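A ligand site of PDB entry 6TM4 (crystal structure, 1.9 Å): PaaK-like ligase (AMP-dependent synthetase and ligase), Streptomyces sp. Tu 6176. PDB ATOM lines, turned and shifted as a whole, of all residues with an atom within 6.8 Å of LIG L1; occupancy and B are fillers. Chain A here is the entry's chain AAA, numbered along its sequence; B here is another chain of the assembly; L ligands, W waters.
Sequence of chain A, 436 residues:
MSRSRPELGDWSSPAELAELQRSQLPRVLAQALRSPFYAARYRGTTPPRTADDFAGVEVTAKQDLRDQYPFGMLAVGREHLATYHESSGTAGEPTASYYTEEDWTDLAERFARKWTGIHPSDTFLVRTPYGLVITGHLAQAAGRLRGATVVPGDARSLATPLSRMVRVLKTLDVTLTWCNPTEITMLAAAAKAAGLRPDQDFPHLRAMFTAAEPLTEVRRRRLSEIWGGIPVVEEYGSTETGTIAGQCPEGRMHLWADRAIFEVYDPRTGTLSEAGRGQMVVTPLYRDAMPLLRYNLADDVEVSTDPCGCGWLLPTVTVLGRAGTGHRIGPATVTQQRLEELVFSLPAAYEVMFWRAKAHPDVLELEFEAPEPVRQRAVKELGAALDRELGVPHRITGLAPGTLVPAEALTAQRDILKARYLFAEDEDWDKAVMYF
O of Thr 135 lies within hydrogen-bond range of NE1 of Trp 178 (3.3 Å).
ND2 of Asn 180 sits at hydrogen-bond distance from OH of Tyr 436 of chain B (2.6 Å).
The backbone NH of Glu 183 sits at hydrogen-bond distance from the side-chain amide oxygen of Asn 180 (2.8 Å).
The backbone carbonyl oxygen (O) of Trp 178 sits at hydrogen-bond distance from the backbone NH (N) of Arg 127 (2.8 Å).
The guanidinium group of Arg 156 sits at hydrogen-bond distance from the backbone carbonyl oxygen of Leu 418 of chain B.
The side-chain hydroxyl of Thr 128 sits at hydrogen-bond distance from the indole nitrogen of Trp 178.
The backbone carbonyl oxygen of Thr 128 sits at hydrogen-bond distance from the backbone NH of Ala 155, 3.4 Å away.
The side-chain amide oxygen of Asn 180 sits close to the side-chain carboxylate of Glu 213.
The side-chain amide nitrogen of Asn 180 sits at hydrogen-bond distance from an oxygen (O2) of LIG L1.
The guanidinium group of Arg 156 lies within salt-bridge range of an oxygen (O1) of LIG L1 (3.4 Å).
The side-chain amino group (NZ) of Lys 419 of chain B is in salt-bridge range of an oxygen (O1) of LG2 L2, at 3.1 Å.
N of Thr 239 is in hydrogen-bond range of O3 of LG2 L2 (3.3 Å).
Water W1 bridges the guanidinium group (NE) of Arg 156 and an oxygen (O1) of LIG L1.
Residues that only touch LIG L1: Thr 128 (3.2 Å), Thr 135 (3.3 Å), Ala 212 (3.4 Å), Trp 178 (3.5 Å), Pro 129 (3.6 Å), Ala 211 (3.8 Å) and Lys 419 of chain B (3.8 Å).
Hydrophobic or aromatic side chains that line LIG L1: Pro 129, Trp 178 and Ala 212.
The nearest printed residue that does not touch LIG L1 is Cys 179 (4.2 Å).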
ATOM      1  N   SER A  88       8.400 -29.638  28.503  1.00  0.00           N
ATOM      2  CA  SER A  88       7.858 -28.630  29.467  1.00  0.00           C
ATOM      3  C   SER A  88       6.331 -28.600  29.313  1.00  0.00           C
ATOM      4  O   SER A  88       5.787 -29.446  28.550  1.00  0.00           O
ATOM      5  CB  SER A  88       8.521 -27.287  29.250  1.00  0.00           C
ATOM      6  OG  SER A  88       8.325 -26.839  27.907  1.00  0.00           O
ATOM      7  N   ARG A 127      22.583 -21.920  30.033  1.00  0.00           N
ATOM      8  CA  ARG A 127      21.753 -21.494  31.190  1.00  0.00           C
ATOM      9  C   ARG A 127      20.299 -21.826  30.879  1.00  0.00           C
ATOM     10  O   ARG A 127      19.458 -20.929  30.913  1.00  0.00           O
ATOM     11  CB  ARG A 127      22.008 -20.015  31.520  1.00  0.00           C
ATOM     12  CG  ARG A 127      21.966 -19.688  33.014  1.00  0.00           C
ATOM     13  CD  ARG A 127      20.636 -20.053  33.623  1.00  0.00           C
ATOM     14  NE  ARG A 127      20.354 -19.341  34.854  1.00  0.00           N
ATOM     15  CZ  ARG A 127      20.712 -19.735  36.074  1.00  0.00           C
ATOM     16  NH1 ARG A 127      20.368 -19.014  37.127  1.00  0.00           N
ATOM     17  NH2 ARG A 127      21.425 -20.844  36.223  1.00  0.00           N
ATOM     18  N   THR A 128      20.037 -23.082  30.540  1.00  0.00           N
ATOM     19  CA  THR A 128      18.697 -23.684  30.362  1.00  0.00           C
ATOM     20  C   THR A 128      18.671 -24.993  31.127  1.00  0.00           C
ATOM     21  O   THR A 128      19.726 -25.478  31.522  1.00  0.00           O
ATOM     22  CB  THR A 128      18.350 -23.908  28.891  1.00  0.00           C
ATOM     23  OG1 THR A 128      19.245 -24.877  28.341  1.00  0.00           O
ATOM     24  CG2 THR A 128      18.413 -22.630  28.093  1.00  0.00           C
ATOM     25  N   PRO A 129      17.495 -25.587  31.394  1.00  0.00           N
ATOM     26  CA  PRO A 129      17.433 -26.769  32.232  1.00  0.00           C
ATOM     27  C   PRO A 129      18.068 -27.988  31.545  1.00  0.00           C
ATOM     28  O   PRO A 129      17.895 -28.143  30.339  1.00  0.00           O
ATOM     29  CB  PRO A 129      15.934 -27.006  32.458  1.00  0.00           C
ATOM     30  CG  PRO A 129      15.309 -25.648  32.209  1.00  0.00           C
ATOM     31  CD  PRO A 129      16.159 -25.065  31.095  1.00  0.00           C
ATOM     32  N   VAL A 133      14.112 -32.187  30.108  1.00  0.00           N
ATOM     33  CA  VAL A 133      13.972 -31.458  28.811  1.00  0.00           C
ATOM     34  C   VAL A 133      15.298 -31.534  28.043  1.00  0.00           C
ATOM     35  O   VAL A 133      16.368 -31.755  28.663  1.00  0.00           O
ATOM     36  CB  VAL A 133      13.515 -29.981  28.995  1.00  0.00           C
ATOM     37  CG1 VAL A 133      12.130 -29.905  29.588  1.00  0.00           C
ATOM     38  CG2 VAL A 133      14.463 -29.180  29.841  1.00  0.00           C
ATOM     39  N   THR A 135      16.816 -29.099  26.330  1.00  0.00           N
ATOM     40  CA  THR A 135      17.382 -27.766  26.040  1.00  0.00           C
ATOM     41  C   THR A 135      18.857 -27.636  26.428  1.00  0.00           C
ATOM     42  O   THR A 135      19.662 -27.168  25.598  1.00  0.00           O
ATOM     43  CB  THR A 135      16.523 -26.687  26.716  1.00  0.00           C
ATOM     44  OG1 THR A 135      15.155 -26.982  26.414  1.00  0.00           O
ATOM     45  CG2 THR A 135      16.886 -25.323  26.214  1.00  0.00           C
ATOM     46  N   ALA A 155      19.492 -24.405  34.719  1.00  0.00           N
ATOM     47  CA  ALA A 155      18.506 -23.349  35.024  1.00  0.00           C
ATOM     48  C   ALA A 155      17.463 -24.028  35.885  1.00  0.00           C
ATOM     49  O   ALA A 155      17.263 -25.263  35.683  1.00  0.00           O
ATOM     50  CB  ALA A 155      17.868 -22.725  33.804  1.00  0.00           C
ATOM     51  N   ARG A 156      16.918 -23.271  36.823  1.00  0.00           N
ATOM     52  CA  ARG A 156      15.892 -23.730  37.790  1.00  0.00           C
ATOM     53  C   ARG A 156      16.537 -24.709  38.766  1.00  0.00           C
ATOM     54  O   ARG A 156      15.843 -25.544  39.297  1.00  0.00           O
ATOM     55  CB  ARG A 156      14.777 -24.421  37.021  1.00  0.00           C
ATOM     56  CG  ARG A 156      14.297 -23.616  35.834  1.00  0.00           C
ATOM     57  CD  ARG A 156      13.064 -24.284  35.282  1.00  0.00           C
ATOM     58  NE  ARG A 156      12.711 -23.695  33.996  1.00  0.00           N
ATOM     59  CZ  ARG A 156      11.472 -23.562  33.534  1.00  0.00           C
ATOM     60  NH1 ARG A 156      10.440 -23.982  34.252  1.00  0.00           N
ATOM     61  NH2 ARG A 156      11.283 -23.013  32.357  1.00  0.00           N
ATOM     62  N   TRP A 178      23.291 -19.139  26.288  1.00  0.00           N
ATOM     63  CA  TRP A 178      22.025 -19.750  25.827  1.00  0.00           C
ATOM     64  C   TRP A 178      21.085 -19.718  27.026  1.00  0.00           C
ATOM     65  O   TRP A 178      21.393 -20.340  28.097  1.00  0.00           O
ATOM     66  CB  TRP A 178      22.291 -21.147  25.308  1.00  0.00           C
ATOM     67  CG  TRP A 178      21.110 -22.055  25.089  1.00  0.00           C
ATOM     68  CD1 TRP A 178      20.915 -23.263  25.700  1.00  0.00           C
ATOM     69  CD2 TRP A 178      20.047 -21.923  24.139  1.00  0.00           C
ATOM     70  NE1 TRP A 178      19.811 -23.894  25.196  1.00  0.00           N
ATOM     71  CE2 TRP A 178      19.243 -23.077  24.253  1.00  0.00           C
ATOM     72  CE3 TRP A 178      19.678 -20.935  23.224  1.00  0.00           C
ATOM     73  CZ2 TRP A 178      18.102 -23.276  23.480  1.00  0.00           C
ATOM     74  CZ3 TRP A 178      18.553 -21.133  22.466  1.00  0.00           C
ATOM     75  CH2 TRP A 178      17.773 -22.286  22.587  1.00  0.00           C
ATOM     76  N   CYS A 179      19.986 -18.988  26.870  1.00  0.00           N
ATOM     77  CA  CYS A 179      18.920 -18.855  27.900  1.00  0.00           C
ATOM     78  C   CYS A 179      17.744 -18.141  27.243  1.00  0.00           C
ATOM     79  O   CYS A 179      17.907 -17.553  26.155  1.00  0.00           O
ATOM     80  CB  CYS A 179      19.432 -18.117  29.134  1.00  0.00           C
ATOM     81  SG  CYS A 179      19.817 -16.368  28.835  1.00  0.00           S
ATOM     82  N   ASN A 180      16.567 -18.260  27.853  1.00  0.00           N
ATOM     83  CA  ASN A 180      15.326 -17.618  27.380  1.00  0.00           C
ATOM     84  C   ASN A 180      15.501 -16.103  27.530  1.00  0.00           C
ATOM     85  O   ASN A 180      16.402 -15.612  28.242  1.00  0.00           O
ATOM     86  CB  ASN A 180      14.120 -18.286  28.053  1.00  0.00           C
ATOM     87  CG  ASN A 180      13.929 -17.898  29.506  1.00  0.00           C
ATOM     88  OD1 ASN A 180      13.906 -16.705  29.804  1.00  0.00           O
ATOM     89  ND2 ASN A 180      13.834 -18.863  30.406  1.00  0.00           N
ATOM     90  N   PRO A 181      14.683 -15.293  26.804  1.00  0.00           N
ATOM     91  CA  PRO A 181      14.828 -13.843  26.818  1.00  0.00           C
ATOM     92  C   PRO A 181      14.595 -13.230  28.216  1.00  0.00           C
ATOM     93  O   PRO A 181      15.275 -12.267  28.573  1.00  0.00           O
ATOM     94  CB  PRO A 181      13.773 -13.350  25.816  1.00  0.00           C
ATOM     95  CG  PRO A 181      13.419 -14.579  24.989  1.00  0.00           C
ATOM     96  CD  PRO A 181      13.606 -15.751  25.917  1.00  0.00           C
ATOM     97  N   GLU A 183      15.440 -14.686  31.053  1.00  0.00           N
ATOM     98  CA  GLU A 183      16.711 -14.951  31.761  1.00  0.00           C
ATOM     99  C   GLU A 183      17.776 -13.932  31.347  1.00  0.00           C
ATOM    100  O   GLU A 183      18.644 -13.586  32.167  1.00  0.00           O
ATOM    101  CB  GLU A 183      17.141 -16.396  31.511  1.00  0.00           C
ATOM    102  CG  GLU A 183      18.186 -16.894  32.478  1.00  0.00           C
ATOM    103  CD  GLU A 183      17.710 -17.055  33.938  1.00  0.00           C
ATOM    104  OE1 GLU A 183      16.512 -17.046  34.189  1.00  0.00           O
ATOM    105  OE2 GLU A 183      18.558 -17.245  34.816  1.00  0.00           O
ATOM    106  N   PHE A 209      22.372 -16.289  22.622  1.00  0.00           N
ATOM    107  CA  PHE A 209      21.429 -17.184  21.918  1.00  0.00           C
ATOM    108  C   PHE A 209      20.195 -17.325  22.799  1.00  0.00           C
ATOM    109  O   PHE A 209      20.329 -17.469  24.042  1.00  0.00           O
ATOM    110  CB  PHE A 209      22.047 -18.553  21.635  1.00  0.00           C
ATOM    111  CG  PHE A 209      23.384 -18.554  20.929  1.00  0.00           C
ATOM    112  CD1 PHE A 209      23.777 -17.516  20.082  1.00  0.00           C
ATOM    113  CD2 PHE A 209      24.246 -19.636  21.078  1.00  0.00           C
ATOM    114  CE1 PHE A 209      24.995 -17.555  19.405  1.00  0.00           C
ATOM    115  CE2 PHE A 209      25.460 -19.662  20.410  1.00  0.00           C
ATOM    116  CZ  PHE A 209      25.827 -18.628  19.580  1.00  0.00           C
ATOM    117  N   THR A 210      19.018 -17.245  22.193  1.00  0.00           N
ATOM    118  CA  THR A 210      17.765 -17.261  22.974  1.00  0.00           C
ATOM    119  C   THR A 210      16.672 -17.909  22.144  1.00  0.00           C
ATOM    120  O   THR A 210      16.820 -17.998  20.917  1.00  0.00           O
ATOM    121  CB  THR A 210      17.432 -15.858  23.460  1.00  0.00           C
ATOM    122  OG1 THR A 210      16.473 -15.994  24.510  1.00  0.00           O
ATOM    123  CG2 THR A 210      16.876 -14.948  22.390  1.00  0.00           C
ATOM    124  N   ALA A 211      15.634 -18.366  22.830  1.00  0.00           N
ATOM    125  CA  ALA A 211      14.420 -19.029  22.269  1.00  0.00           C
ATOM    126  C   ALA A 211      13.419 -19.203  23.415  1.00  0.00           C
ATOM    127  O   ALA A 211      13.812 -18.879  24.561  1.00  0.00           O
ATOM    128  CB  ALA A 211      14.785 -20.375  21.716  1.00  0.00           C
ATOM    129  N   ALA A 212      12.259 -19.795  23.130  1.00  0.00           N
ATOM    130  CA  ALA A 212      11.310 -20.409  24.089  1.00  0.00           C
ATOM    131  C   ALA A 212      10.225 -19.408  24.534  1.00  0.00           C
ATOM    132  O   ALA A 212       9.325 -19.823  25.305  1.00  0.00           O
ATOM    133  CB  ALA A 212      12.033 -20.961  25.290  1.00  0.00           C
ATOM    134  N   GLU A 213      10.336 -18.137  24.117  1.00  0.00           N
ATOM    135  CA  GLU A 213       9.304 -17.095  24.313  1.00  0.00           C
ATOM    136  C   GLU A 213       9.085 -16.410  22.986  1.00  0.00           C
ATOM    137  O   GLU A 213      10.048 -16.126  22.288  1.00  0.00           O
ATOM    138  CB  GLU A 213       9.717 -15.981  25.289  1.00  0.00           C
ATOM    139  CG  GLU A 213       9.669 -16.340  26.762  1.00  0.00           C
ATOM    140  CD  GLU A 213      10.206 -15.256  27.676  1.00  0.00           C
ATOM    141  OE1 GLU A 213      11.134 -15.540  28.492  1.00  0.00           O
ATOM    142  OE2 GLU A 213       9.690 -14.110  27.569  1.00  0.00           O
ATOM    143  N   THR A 239      10.664 -28.616  22.701  1.00  0.00           N
ATOM    144  CA  THR A 239      11.262 -29.677  23.541  1.00  0.00           C
ATOM    145  C   THR A 239      11.238 -31.019  22.785  1.00  0.00           C
ATOM    146  O   THR A 239      12.085 -31.835  23.105  1.00  0.00           O
ATOM    147  CB  THR A 239      10.564 -29.611  24.904  1.00  0.00           C
ATOM    148  OG1 THR A 239       9.188 -29.384  24.655  1.00  0.00           O
ATOM    149  CG2 THR A 239      11.066 -28.454  25.745  1.00  0.00           C
ATOM    150  N   ILE B 417       6.505 -27.376  34.265  1.00  0.00           N
ATOM    151  CA  ILE B 417       7.719 -26.659  33.801  1.00  0.00           C
ATOM    152  C   ILE B 417       7.231 -25.482  32.964  1.00  0.00           C
ATOM    153  O   ILE B 417       7.032 -25.674  31.749  1.00  0.00           O
ATOM    154  CB  ILE B 417       8.697 -27.594  33.042  1.00  0.00           C
ATOM    155  CG1 ILE B 417       8.998 -28.876  33.832  1.00  0.00           C
ATOM    156  CG2 ILE B 417       9.983 -26.859  32.670  1.00  0.00           C
ATOM    157  CD1 ILE B 417       9.766 -29.917  33.020  1.00  0.00           C
ATOM    158  N   LEU B 418       6.954 -24.332  33.600  1.00  0.00           N
ATOM    159  CA  LEU B 418       6.362 -23.142  32.938  1.00  0.00           C
ATOM    160  C   LEU B 418       7.456 -22.274  32.309  1.00  0.00           C
ATOM    161  O   LEU B 418       8.638 -22.408  32.679  1.00  0.00           O
ATOM    162  CB  LEU B 418       5.543 -22.354  33.951  1.00  0.00           C
ATOM    163  CG  LEU B 418       4.366 -23.109  34.544  1.00  0.00           C
ATOM    164  CD1 LEU B 418       3.768 -22.371  35.730  1.00  0.00           C
ATOM    165  CD2 LEU B 418       3.309 -23.390  33.470  1.00  0.00           C
ATOM    166  N   LYS B 419       7.048 -21.440  31.361  1.00  0.00           N
ATOM    167  CA  LYS B 419       7.880 -20.381  30.762  1.00  0.00           C
ATOM    168  C   LYS B 419       7.292 -19.057  31.221  1.00  0.00           C
ATOM    169  O   LYS B 419       6.107 -19.060  31.606  1.00  0.00           O
ATOM    170  CB  LYS B 419       7.933 -20.595  29.249  1.00  0.00           C
ATOM    171  CG  LYS B 419       8.757 -21.815  28.867  1.00  0.00           C
ATOM    172  CD  LYS B 419       8.437 -22.450  27.522  1.00  0.00           C
ATOM    173  CE  LYS B 419       9.255 -23.704  27.297  1.00  0.00           C
ATOM    174  NZ  LYS B 419       9.461 -24.024  25.856  1.00  0.00           N
ATOM    175  N   TYR B 436       8.752 -17.586  37.279  1.00  0.00           N
ATOM    176  CA  TYR B 436       7.916 -18.666  36.661  1.00  0.00           C
ATOM    177  C   TYR B 436       8.435 -20.061  37.044  1.00  0.00           C
ATOM    178  O   TYR B 436       7.756 -21.057  36.661  1.00  0.00           O
ATOM    179  CB  TYR B 436       7.836 -18.491  35.142  1.00  0.00           C
ATOM    180  CG  TYR B 436       9.176 -18.370  34.452  1.00  0.00           C
ATOM    181  CD1 TYR B 436       9.778 -17.134  34.289  1.00  0.00           C
ATOM    182  CD2 TYR B 436       9.875 -19.488  34.022  1.00  0.00           C
ATOM    183  CE1 TYR B 436      11.027 -16.999  33.705  1.00  0.00           C
ATOM    184  CE2 TYR B 436      11.122 -19.371  33.422  1.00  0.00           C
ATOM    185  CZ  TYR B 436      11.696 -18.110  33.234  1.00  0.00           C
ATOM    186  OH  TYR B 436      12.952 -17.960  32.682  1.00  0.00           O
ATOM    187  N   PHE B 437       9.568 -20.151  37.760  1.00  0.00           N
ATOM    188  CA  PHE B 437      10.271 -21.432  38.064  1.00  0.00           C
ATOM    189  C   PHE B 437       9.422 -22.281  39.022  1.00  0.00           C
ATOM    190  O   PHE B 437       8.544 -21.743  39.743  1.00  0.00           O
ATOM    191  CB  PHE B 437      11.649 -21.223  38.701  1.00  0.00           C
ATOM    192  CG  PHE B 437      12.763 -20.682  37.826  1.00  0.00           C
ATOM    193  CD1 PHE B 437      12.605 -20.516  36.453  1.00  0.00           C
ATOM    194  CD2 PHE B 437      13.995 -20.363  38.396  1.00  0.00           C
ATOM    195  CE1 PHE B 437      13.645 -20.008  35.688  1.00  0.00           C
ATOM    196  CE2 PHE B 437      15.033 -19.869  37.628  1.00  0.00           C
ATOM    197  CZ  PHE B 437      14.862 -19.703  36.270  1.00  0.00           C
ATOM    198  OXT PHE B 437       9.648 -23.522  39.071  1.00  0.00           O
HETATM  199  C1  LIG L   1      14.507 -22.151  29.245  1.00  0.00           C
HETATM  200  O1  LIG L   1      13.619 -22.749  29.881  1.00  0.00           O
HETATM  201  O2  LIG L   1      15.307 -21.379  29.782  1.00  0.00           O
HETATM  202  C2  LIG L   1      14.641 -22.411  27.765  1.00  0.00           C
HETATM  203  C3  LIG L   1      13.767 -23.445  27.221  1.00  0.00           C
HETATM  204  C4  LIG L   1      13.845 -23.743  25.853  1.00  0.00           C
HETATM  205  C5  LIG L   1      14.751 -23.049  25.030  1.00  0.00           C
HETATM  206  C6  LIG L   1      15.592 -22.056  25.560  1.00  0.00           C
HETATM  207  C7  LIG L   1      15.534 -21.749  26.932  1.00  0.00           C
HETATM  208  O3  LIG L   1      12.929 -24.055  28.103  1.00  0.00           O
HETATM  209  C1  LG2 L   2      11.880 -24.310  22.871  1.00  0.00           C
HETATM  210  O1  LG2 L   2      11.500 -25.096  23.766  1.00  0.00           O
HETATM  211  O2  LG2 L   2      11.214 -23.279  22.562  1.00  0.00           O
HETATM  212  C2  LG2 L   2      13.157 -24.689  22.171  1.00  0.00           C
HETATM  213  C3  LG2 L   2      13.816 -25.956  22.530  1.00  0.00           C
HETATM  214  C4  LG2 L   2      15.003 -26.347  21.924  1.00  0.00           C
HETATM  215  C5  LG2 L   2      15.546 -25.538  20.947  1.00  0.00           C
HETATM  216  C6  LG2 L   2      14.929 -24.342  20.600  1.00  0.00           C
HETATM  217  C7  LG2 L   2      13.745 -23.920  21.194  1.00  0.00           C
HETATM  218  O3  LG2 L   2      13.241 -26.719  23.452  1.00  0.00           O
HETATM  219  O   HOH W   1      14.451 -21.920  32.536  1.00  0.00           O
